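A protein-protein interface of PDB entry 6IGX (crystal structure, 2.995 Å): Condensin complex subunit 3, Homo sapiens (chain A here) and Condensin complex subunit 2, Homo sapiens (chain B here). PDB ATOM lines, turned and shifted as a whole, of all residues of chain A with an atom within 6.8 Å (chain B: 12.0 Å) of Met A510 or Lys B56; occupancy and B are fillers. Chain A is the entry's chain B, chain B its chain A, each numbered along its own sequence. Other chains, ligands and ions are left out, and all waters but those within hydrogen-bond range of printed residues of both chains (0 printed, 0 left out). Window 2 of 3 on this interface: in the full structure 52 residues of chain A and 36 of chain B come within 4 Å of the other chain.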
ATOM      1  N   ASP A 469      20.678 -25.306 -13.782  1.00  0.00           N
ATOM      2  CA  ASP A 469      19.820 -25.577 -14.934  1.00  0.00           C
ATOM      3  C   ASP A 469      20.475 -26.502 -15.961  1.00  0.00           C
ATOM      4  O   ASP A 469      19.804 -27.340 -16.561  1.00  0.00           O
ATOM      5  CB  ASP A 469      19.374 -24.262 -15.581  1.00  0.00           C
ATOM      6  CG  ASP A 469      18.234 -23.604 -14.814  1.00  0.00           C
ATOM      7  OD1 ASP A 469      18.035 -23.967 -13.636  1.00  0.00           O
ATOM      8  OD2 ASP A 469      17.519 -22.752 -15.382  1.00  0.00           O
ATOM      9  N   ASN A 470      21.779 -26.343 -16.170  1.00  0.00           N
ATOM     10  CA  ASN A 470      22.492 -27.190 -17.121  1.00  0.00           C
ATOM     11  C   ASN A 470      22.740 -28.578 -16.541  1.00  0.00           C
ATOM     12  O   ASN A 470      22.685 -29.574 -17.257  1.00  0.00           O
ATOM     13  CB  ASN A 470      23.819 -26.551 -17.537  1.00  0.00           C
ATOM     14  CG  ASN A 470      23.643 -25.456 -18.572  1.00  0.00           C
ATOM     15  OD1 ASN A 470      22.700 -25.481 -19.366  1.00  0.00           O
ATOM     16  ND2 ASN A 470      24.556 -24.492 -18.575  1.00  0.00           N
ATOM     17  N   ARG A 472      20.781 -29.956 -14.398  1.00  0.00           N
ATOM     18  CA  ARG A 472      19.471 -30.595 -14.369  1.00  0.00           C
ATOM     19  C   ARG A 472      19.173 -31.202 -15.737  1.00  0.00           C
ATOM     20  O   ARG A 472      18.768 -32.359 -15.835  1.00  0.00           O
ATOM     21  CB  ARG A 472      18.380 -29.594 -13.972  1.00  0.00           C
ATOM     22  CG  ARG A 472      18.556 -28.997 -12.583  1.00  0.00           C
ATOM     23  CD  ARG A 472      17.662 -27.784 -12.374  1.00  0.00           C
ATOM     24  NE  ARG A 472      17.937 -27.119 -11.102  1.00  0.00           N
ATOM     25  CZ  ARG A 472      17.399 -25.962 -10.730  1.00  0.00           C
ATOM     26  NH1 ARG A 472      16.554 -25.332 -11.535  1.00  0.00           N
ATOM     27  NH2 ARG A 472      17.709 -25.432  -9.555  1.00  0.00           N
ATOM     28  N   THR A 473      19.380 -30.412 -16.787  1.00  0.00           N
ATOM     29  CA  THR A 473      19.159 -30.872 -18.155  1.00  0.00           C
ATOM     30  C   THR A 473      20.025 -32.082 -18.504  1.00  0.00           C
ATOM     31  O   THR A 473      19.634 -32.917 -19.320  1.00  0.00           O
ATOM     32  CB  THR A 473      19.439 -29.751 -19.177  1.00  0.00           C
ATOM     33  OG1 THR A 473      20.777 -29.268 -19.008  1.00  0.00           O
ATOM     34  CG2 THR A 473      18.464 -28.600 -18.988  1.00  0.00           C
ATOM     35  N   TYR A 504       8.837 -32.101 -19.070  1.00  0.00           N
ATOM     36  CA  TYR A 504       7.911 -31.076 -18.602  1.00  0.00           C
ATOM     37  C   TYR A 504       8.373 -30.486 -17.277  1.00  0.00           C
ATOM     38  O   TYR A 504       8.523 -29.271 -17.143  1.00  0.00           O
ATOM     39  CB  TYR A 504       6.499 -31.648 -18.455  1.00  0.00           C
ATOM     40  CG  TYR A 504       5.426 -30.599 -18.242  1.00  0.00           C
ATOM     41  CD1 TYR A 504       5.676 -29.257 -18.501  1.00  0.00           C
ATOM     42  CD2 TYR A 504       4.168 -30.951 -17.772  1.00  0.00           C
ATOM     43  CE1 TYR A 504       4.700 -28.297 -18.304  1.00  0.00           C
ATOM     44  CE2 TYR A 504       3.184 -29.997 -17.571  1.00  0.00           C
ATOM     45  CZ  TYR A 504       3.456 -28.672 -17.839  1.00  0.00           C
ATOM     46  OH  TYR A 504       2.483 -27.718 -17.641  1.00  0.00           O
ATOM     47  N   GLU A 505       8.594 -31.357 -16.299  1.00  0.00           N
ATOM     48  CA  GLU A 505       8.959 -30.927 -14.957  1.00  0.00           C
ATOM     49  C   GLU A 505      10.321 -30.235 -14.955  1.00  0.00           C
ATOM     50  O   GLU A 505      10.681 -29.553 -13.995  1.00  0.00           O
ATOM     51  CB  GLU A 505       8.964 -32.121 -14.002  1.00  0.00           C
ATOM     52  CG  GLU A 505       7.581 -32.502 -13.501  1.00  0.00           C
ATOM     53  CD  GLU A 505       6.990 -31.462 -12.572  1.00  0.00           C
ATOM     54  OE1 GLU A 505       7.768 -30.732 -11.921  1.00  0.00           O
ATOM     55  OE2 GLU A 505       5.746 -31.372 -12.495  1.00  0.00           O
ATOM     56  N   LEU A 506      11.071 -30.417 -16.037  1.00  0.00           N
ATOM     57  CA  LEU A 506      12.349 -29.738 -16.210  1.00  0.00           C
ATOM     58  C   LEU A 506      12.153 -28.332 -16.763  1.00  0.00           C
ATOM     59  O   LEU A 506      12.795 -27.382 -16.318  1.00  0.00           O
ATOM     60  CB  LEU A 506      13.261 -30.537 -17.143  1.00  0.00           C
ATOM     61  CG  LEU A 506      14.586 -29.864 -17.515  1.00  0.00           C
ATOM     62  CD1 LEU A 506      15.522 -29.794 -16.316  1.00  0.00           C
ATOM     63  CD2 LEU A 506      15.251 -30.575 -18.684  1.00  0.00           C
ATOM     64  N   LEU A 507      11.256 -28.211 -17.737  1.00  0.00           N
ATOM     65  CA  LEU A 507      11.018 -26.944 -18.419  1.00  0.00           C
ATOM     66  C   LEU A 507      10.318 -25.918 -17.534  1.00  0.00           C
ATOM     67  O   LEU A 507      10.616 -24.725 -17.603  1.00  0.00           O
ATOM     68  CB  LEU A 507      10.205 -27.173 -19.695  1.00  0.00           C
ATOM     69  CG  LEU A 507      11.006 -27.725 -20.877  1.00  0.00           C
ATOM     70  CD1 LEU A 507      10.112 -28.503 -21.828  1.00  0.00           C
ATOM     71  CD2 LEU A 507      11.728 -26.601 -21.609  1.00  0.00           C
ATOM     72  N   LYS A 508       9.387 -26.379 -16.706  1.00  0.00           N
ATOM     73  CA  LYS A 508       8.595 -25.468 -15.890  1.00  0.00           C
ATOM     74  C   LYS A 508       9.407 -24.850 -14.753  1.00  0.00           C
ATOM     75  O   LYS A 508       9.180 -23.700 -14.382  1.00  0.00           O
ATOM     76  CB  LYS A 508       7.367 -26.188 -15.324  1.00  0.00           C
ATOM     77  CG  LYS A 508       7.656 -27.090 -14.136  1.00  0.00           C
ATOM     78  CD  LYS A 508       6.380 -27.741 -13.623  1.00  0.00           C
ATOM     79  CE  LYS A 508       5.599 -28.392 -14.755  1.00  0.00           C
ATOM     80  NZ  LYS A 508       4.425 -29.161 -14.253  1.00  0.00           N
ATOM     81  N   GLN A 509      10.347 -25.610 -14.200  1.00  0.00           N
ATOM     82  CA  GLN A 509      11.196 -25.103 -13.124  1.00  0.00           C
ATOM     83  C   GLN A 509      12.421 -24.358 -13.657  1.00  0.00           C
ATOM     84  O   GLN A 509      13.179 -23.766 -12.889  1.00  0.00           O
ATOM     85  CB  GLN A 509      11.651 -26.240 -12.208  1.00  0.00           C
ATOM     86  CG  GLN A 509      12.242 -25.756 -10.888  1.00  0.00           C
ATOM     87  CD  GLN A 509      13.424 -26.585 -10.423  1.00  0.00           C
ATOM     88  OE1 GLN A 509      14.001 -27.353 -11.194  1.00  0.00           O
ATOM     89  NE2 GLN A 509      13.790 -26.432  -9.155  1.00  0.00           N
ATOM     90  N   MET A 510      12.610 -24.388 -14.972  1.00  0.00           N
ATOM     91  CA  MET A 510      13.769 -23.753 -15.587  1.00  0.00           C
ATOM     92  C   MET A 510      13.577 -22.248 -15.742  1.00  0.00           C
ATOM     93  O   MET A 510      12.544 -21.791 -16.231  1.00  0.00           O
ATOM     94  CB  MET A 510      14.062 -24.382 -16.950  1.00  0.00           C
ATOM     95  CG  MET A 510      15.285 -23.806 -17.644  1.00  0.00           C
ATOM     96  SD  MET A 510      15.671 -24.647 -19.191  1.00  0.00           S
ATOM     97  CE  MET A 510      15.920 -26.323 -18.611  1.00  0.00           C
ATOM     98  N   SER A 511      14.580 -21.483 -15.318  1.00  0.00           N
ATOM     99  CA  SER A 511      14.514 -20.027 -15.387  1.00  0.00           C
ATOM    100  C   SER A 511      14.695 -19.569 -16.830  1.00  0.00           C
ATOM    101  O   SER A 511      15.362 -20.235 -17.620  1.00  0.00           O
ATOM    102  CB  SER A 511      15.579 -19.395 -14.489  1.00  0.00           C
ATOM    103  OG  SER A 511      15.687 -20.098 -13.262  1.00  0.00           O
ATOM    104  N   ILE A 512      14.101 -18.430 -17.163  1.00  0.00           N
ATOM    105  CA  ILE A 512      14.082 -17.950 -18.540  1.00  0.00           C
ATOM    106  C   ILE A 512      15.469 -17.613 -19.088  1.00  0.00           C
ATOM    107  O   ILE A 512      15.679 -17.640 -20.302  1.00  0.00           O
ATOM    108  CB  ILE A 512      13.164 -16.712 -18.682  1.00  0.00           C
ATOM    109  CG1 ILE A 512      11.709 -17.102 -18.413  1.00  0.00           C
ATOM    110  CG2 ILE A 512      13.289 -16.092 -20.068  1.00  0.00           C
ATOM    111  CD1 ILE A 512      11.213 -18.263 -19.263  1.00  0.00           C
ATOM    112  N   SER A 513      16.416 -17.301 -18.205  1.00  0.00           N
ATOM    113  CA  SER A 513      17.722 -16.828 -18.659  1.00  0.00           C
ATOM    114  C   SER A 513      18.444 -17.871 -19.510  1.00  0.00           C
ATOM    115  O   SER A 513      18.982 -17.553 -20.570  1.00  0.00           O
ATOM    116  CB  SER A 513      18.598 -16.441 -17.463  1.00  0.00           C
ATOM    117  OG  SER A 513      18.976 -17.582 -16.708  1.00  0.00           O
ATOM    118  N   THR A 514      18.449 -19.114 -19.034  1.00  0.00           N
ATOM    119  CA  THR A 514      19.218 -20.192 -19.657  1.00  0.00           C
ATOM    120  C   THR A 514      18.405 -20.907 -20.733  1.00  0.00           C
ATOM    121  O   THR A 514      18.532 -22.118 -20.918  1.00  0.00           O
ATOM    122  CB  THR A 514      19.697 -21.216 -18.620  1.00  0.00           C
ATOM    123  OG1 THR A 514      20.221 -22.367 -19.292  1.00  0.00           O
ATOM    124  CG2 THR A 514      18.548 -21.636 -17.741  1.00  0.00           C
ATOM    125  N   GLY A 515      17.556 -20.151 -21.417  1.00  0.00           N
ATOM    126  CA  GLY A 515      16.674 -20.670 -22.448  1.00  0.00           C
ATOM    127  C   GLY A 515      17.249 -21.547 -23.546  1.00  0.00           C
ATOM    128  O   GLY A 515      18.106 -21.109 -24.309  1.00  0.00           O
ATOM    129  N   LEU A 516      16.785 -22.791 -23.618  1.00  0.00           N
ATOM    130  CA  LEU A 516      17.112 -23.672 -24.740  1.00  0.00           C
ATOM    131  C   LEU A 516      18.594 -24.000 -24.911  1.00  0.00           C
ATOM    132  O   LEU A 516      19.142 -23.841 -26.001  1.00  0.00           O
ATOM    133  CB  LEU A 516      16.593 -23.065 -26.047  1.00  0.00           C
ATOM    134  CG  LEU A 516      15.082 -23.130 -26.289  1.00  0.00           C
ATOM    135  CD1 LEU A 516      14.772 -22.802 -27.741  1.00  0.00           C
ATOM    136  CD2 LEU A 516      14.533 -24.499 -25.916  1.00  0.00           C
ATOM    137  N   SER A 517      19.245 -24.421 -23.829  1.00  0.00           N
ATOM    138  CA  SER A 517      20.608 -24.942 -23.907  1.00  0.00           C
ATOM    139  C   SER A 517      20.717 -25.971 -25.027  1.00  0.00           C
ATOM    140  O   SER A 517      19.833 -26.816 -25.179  1.00  0.00           O
ATOM    141  CB  SER A 517      21.028 -25.569 -22.577  1.00  0.00           C
ATOM    142  OG  SER A 517      20.091 -26.546 -22.159  1.00  0.00           O
ATOM    143  N   MET A 520      19.239 -29.079 -24.627  1.00  0.00           N
ATOM    144  CA  MET A 520      17.780 -29.124 -24.664  1.00  0.00           C
ATOM    145  C   MET A 520      17.274 -29.345 -26.082  1.00  0.00           C
ATOM    146  O   MET A 520      16.344 -30.123 -26.302  1.00  0.00           O
ATOM    147  CB  MET A 520      17.187 -27.833 -24.093  1.00  0.00           C
ATOM    148  CG  MET A 520      16.916 -27.875 -22.598  1.00  0.00           C
ATOM    149  SD  MET A 520      15.523 -28.936 -22.160  1.00  0.00           S
ATOM    150  CE  MET A 520      14.571 -28.895 -23.677  1.00  0.00           C
ATOM    151  N   CYS A 549       6.450 -24.820 -23.346  1.00  0.00           N
ATOM    152  CA  CYS A 549       7.392 -24.411 -22.312  1.00  0.00           C
ATOM    153  C   CYS A 549       8.720 -24.009 -22.940  1.00  0.00           C
ATOM    154  O   CYS A 549       9.430 -23.150 -22.420  1.00  0.00           O
ATOM    155  CB  CYS A 549       7.599 -25.532 -21.294  1.00  0.00           C
ATOM    156  SG  CYS A 549       6.385 -25.541 -19.958  1.00  0.00           S
ATOM    157  N   LEU A 552       8.589 -20.547 -24.656  1.00  0.00           N
ATOM    158  CA  LEU A 552       8.672 -19.484 -23.659  1.00  0.00           C
ATOM    159  C   LEU A 552      10.108 -19.105 -23.399  1.00  0.00           C
ATOM    160  O   LEU A 552      10.395 -18.063 -22.810  1.00  0.00           O
ATOM    161  CB  LEU A 552       8.044 -19.922 -22.337  1.00  0.00           C
ATOM    162  CG  LEU A 552       6.530 -20.056 -22.261  1.00  0.00           C
ATOM    163  CD1 LEU A 552       6.119 -20.653 -20.915  1.00  0.00           C
ATOM    164  CD2 LEU A 552       5.876 -18.700 -22.505  1.00  0.00           C
ATOM    165  N   GLN A 553      11.011 -19.979 -23.820  1.00  0.00           N
ATOM    166  CA  GLN A 553      12.416 -19.822 -23.506  1.00  0.00           C
ATOM    167  C   GLN A 553      13.083 -18.929 -24.553  1.00  0.00           C
ATOM    168  O   GLN A 553      13.778 -17.971 -24.220  1.00  0.00           O
ATOM    169  CB  GLN A 553      13.085 -21.196 -23.435  1.00  0.00           C
ATOM    170  CG  GLN A 553      13.746 -21.480 -22.100  1.00  0.00           C
ATOM    171  CD  GLN A 553      12.753 -21.390 -20.952  1.00  0.00           C
ATOM    172  OE1 GLN A 553      11.541 -21.465 -21.163  1.00  0.00           O
ATOM    173  NE2 GLN A 553      13.259 -21.237 -19.736  1.00  0.00           N
ATOM    174  N   ASP A 586      -0.097 -18.490 -23.201  1.00  0.00           N
ATOM    175  CA  ASP A 586       1.061 -18.102 -22.403  1.00  0.00           C
ATOM    176  C   ASP A 586       2.122 -17.449 -23.277  1.00  0.00           C
ATOM    177  O   ASP A 586       2.899 -16.619 -22.809  1.00  0.00           O
ATOM    178  CB  ASP A 586       1.645 -19.308 -21.664  1.00  0.00           C
ATOM    179  CG  ASP A 586       0.850 -19.670 -20.423  1.00  0.00           C
ATOM    180  OD1 ASP A 586      -0.312 -19.227 -20.309  1.00  0.00           O
ATOM    181  OD2 ASP A 586       1.390 -20.391 -19.559  1.00  0.00           O
ATOM    182  N   ASP B  48      -5.442 -11.923  -9.901  1.00  0.00           N
ATOM    183  CA  ASP B  48      -4.046 -12.249 -10.170  1.00  0.00           C
ATOM    184  C   ASP B  48      -3.916 -13.405 -11.158  1.00  0.00           C
ATOM    185  O   ASP B  48      -2.928 -13.497 -11.886  1.00  0.00           O
ATOM    186  CB  ASP B  48      -3.320 -12.594  -8.869  1.00  0.00           C
ATOM    187  CG  ASP B  48      -3.393 -11.478  -7.846  1.00  0.00           C
ATOM    188  OD1 ASP B  48      -3.318 -10.296  -8.241  1.00  0.00           O
ATOM    189  OD2 ASP B  48      -3.529 -11.784  -6.642  1.00  0.00           O
ATOM    190  N   THR B  49      -4.912 -14.286 -11.182  1.00  0.00           N
ATOM    191  CA  THR B  49      -4.914 -15.393 -12.132  1.00  0.00           C
ATOM    192  C   THR B  49      -5.084 -14.869 -13.556  1.00  0.00           C
ATOM    193  O   THR B  49      -4.769 -15.560 -14.526  1.00  0.00           O
ATOM    194  CB  THR B  49      -6.027 -16.413 -11.821  1.00  0.00           C
ATOM    195  OG1 THR B  49      -7.284 -15.734 -11.709  1.00  0.00           O
ATOM    196  CG2 THR B  49      -5.737 -17.138 -10.519  1.00  0.00           C
ATOM    197  N   VAL B  51      -3.388 -12.470 -14.732  1.00  0.00           N
ATOM    198  CA  VAL B  51      -2.068 -12.069 -15.207  1.00  0.00           C
ATOM    199  C   VAL B  51      -1.056 -13.214 -15.122  1.00  0.00           C
ATOM    200  O   VAL B  51       0.127 -13.031 -15.412  1.00  0.00           O
ATOM    201  CB  VAL B  51      -1.539 -10.862 -14.409  1.00  0.00           C
ATOM    202  CG1 VAL B  51      -0.845 -11.330 -13.139  1.00  0.00           C
ATOM    203  CG2 VAL B  51      -0.597 -10.030 -15.263  1.00  0.00           C
ATOM    204  N   GLN B  52      -1.528 -14.390 -14.719  1.00  0.00           N
ATOM    205  CA  GLN B  52      -0.668 -15.557 -14.514  1.00  0.00           C
ATOM    206  C   GLN B  52      -0.693 -16.541 -15.689  1.00  0.00           C
ATOM    207  O   GLN B  52      -1.646 -16.571 -16.469  1.00  0.00           O
ATOM    208  CB  GLN B  52      -1.047 -16.269 -13.216  1.00  0.00           C
ATOM    209  CG  GLN B  52      -0.290 -15.738 -12.008  1.00  0.00           C
ATOM    210  CD  GLN B  52      -0.804 -16.295 -10.698  1.00  0.00           C
ATOM    211  OE1 GLN B  52      -1.575 -17.254 -10.677  1.00  0.00           O
ATOM    212  NE2 GLN B  52      -0.375 -15.694  -9.593  1.00  0.00           N
ATOM    213  N   LEU B  53       0.368 -17.339 -15.803  1.00  0.00           N
ATOM    214  CA  LEU B  53       0.523 -18.302 -16.894  1.00  0.00           C
ATOM    215  C   LEU B  53      -0.040 -19.684 -16.559  1.00  0.00           C
ATOM    216  O   LEU B  53      -0.262 -20.011 -15.393  1.00  0.00           O
ATOM    217  CB  LEU B  53       2.002 -18.448 -17.276  1.00  0.00           C
ATOM    218  CG  LEU B  53       2.861 -17.261 -17.732  1.00  0.00           C
ATOM    219  CD1 LEU B  53       2.546 -16.892 -19.177  1.00  0.00           C
ATOM    220  CD2 LEU B  53       2.720 -16.048 -16.820  1.00  0.00           C
ATOM    221  N   HIS B  54      -0.268 -20.486 -17.596  1.00  0.00           N
ATOM    222  CA  HIS B  54      -0.823 -21.831 -17.448  1.00  0.00           C
ATOM    223  C   HIS B  54       0.264 -22.881 -17.245  1.00  0.00           C
ATOM    224  O   HIS B  54       0.014 -23.939 -16.668  1.00  0.00           O
ATOM    225  CB  HIS B  54      -1.659 -22.217 -18.673  1.00  0.00           C
ATOM    226  CG  HIS B  54      -2.921 -21.427 -18.830  1.00  0.00           C
ATOM    227  ND1 HIS B  54      -3.970 -21.518 -17.941  1.00  0.00           N
ATOM    228  CD2 HIS B  54      -3.308 -20.545 -19.781  1.00  0.00           C
ATOM    229  CE1 HIS B  54      -4.947 -20.719 -18.334  1.00  0.00           C
ATOM    230  NE2 HIS B  54      -4.570 -20.117 -19.448  1.00  0.00           N
ATOM    231  N   LEU B  55       1.467 -22.587 -17.729  1.00  0.00           N
ATOM    232  CA  LEU B  55       2.535 -23.581 -17.782  1.00  0.00           C
ATOM    233  C   LEU B  55       3.501 -23.483 -16.604  1.00  0.00           C
ATOM    234  O   LEU B  55       4.364 -24.344 -16.431  1.00  0.00           O
ATOM    235  CB  LEU B  55       3.310 -23.444 -19.095  1.00  0.00           C
ATOM    236  CG  LEU B  55       2.517 -23.702 -20.378  1.00  0.00           C
ATOM    237  CD1 LEU B  55       3.384 -23.464 -21.604  1.00  0.00           C
ATOM    238  CD2 LEU B  55       1.946 -25.111 -20.384  1.00  0.00           C
ATOM    239  N   LYS B  56       3.359 -22.438 -15.795  1.00  0.00           N
ATOM    240  CA  LYS B  56       4.256 -22.235 -14.662  1.00  0.00           C
ATOM    241  C   LYS B  56       3.486 -21.877 -13.393  1.00  0.00           C
ATOM    242  O   LYS B  56       3.967 -22.098 -12.280  1.00  0.00           O
ATOM    243  CB  LYS B  56       5.277 -21.143 -14.984  1.00  0.00           C
ATOM    244  CG  LYS B  56       6.161 -21.464 -16.179  1.00  0.00           C
ATOM    245  CD  LYS B  56       7.309 -20.479 -16.304  1.00  0.00           C
ATOM    246  CE  LYS B  56       8.114 -20.730 -17.569  1.00  0.00           C
ATOM    247  NZ  LYS B  56       8.849 -22.025 -17.517  1.00  0.00           N
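Of the printed residues of chain B, Met A510 touches Lys B56.
Lys B56 touches four residues of chain A.
No residue of chain B comes within 4 Å of Asp A469.
No residue of chain B comes within 4 Å of Thr A473.
No residue of chain B comes within 4 Å of Leu A506.
Of the printed residues of chain B, Leu A507 touches Lys B56 (3.2 Å).
Of chain B, only Leu B55 (3.7 Å) and Lys B56 (3.6 Å) come within 4 Å of Lys A508.
No residue of chain B comes within 4 Å of Ser A511.
No residue of chain B comes within 4 Å of Gly A515.
No residue of chain B comes within 4 Å of Ser A517.
Cys A549 touches just one residue of chain B: Leu B55 (3.8 Å).
Printed residues of chain A within 4 Å of Leu B55: Tyr A504 (3.8 Å), Lys A508 (3.7 Å), Cys A549 (3.8 Å), Leu A552 (3.98 Å) and Asp A586 (2.9 Å).
Printed residues of chain B within 4 Å of Leu A552: Leu B55 (3.98 Å) and Lys B56 (3.9 Å).
The nearest residue of chain B that does not touch Met A510 is Leu B55 (8.4 Å).
OE2 of Glu A505 lies within salt-bridge range of NZ of Lys A508 (3.1 Å).
OE1 of Gln A553 sits close to O of Cys A549 (3.0 Å).
Printed residues of chain B that touch a printed residue of chain A: Leu B53, His B54, Leu B55 and Lys B56.
Hydrophobic or aromatic side chains of chain B within 4 Å of the printed part of chain A: Leu B53, His B54 and Leu B55.
Among the printed residues, no Asp or Glu carboxylate lies within 4 Å of a Lys or Arg side-chain nitrogen of the other chain.
The backbone carbonyl oxygen of Leu A507 lies within hydrogen-bond range of the side-chain amino group of Lys B56, 3.2 Å away.
The backbone NH of His B54 is in hydrogen-bond range of the side-chain carboxylate of Asp A586.
The backbone NH of Leu B55 lies within hydrogen-bond range of the side-chain carboxylate of Asp A586 (2.9 Å).
Among the printed residues, pairs that only touch across the chains: Asp A586 with Leu B53 (3.1 Å), Lys A508 with Lys B56 (3.6 Å), Lys A508 with Leu B55 (3.7 Å), Cys A549 with Leu B55 (3.8 Å), Tyr A504 with Leu B55 (3.8 Å), Leu A552 with Lys B56 (3.9 Å), Met A510 with Lys B56 (3.9 Å) and Leu A552 with Leu B55 (3.98 Å).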
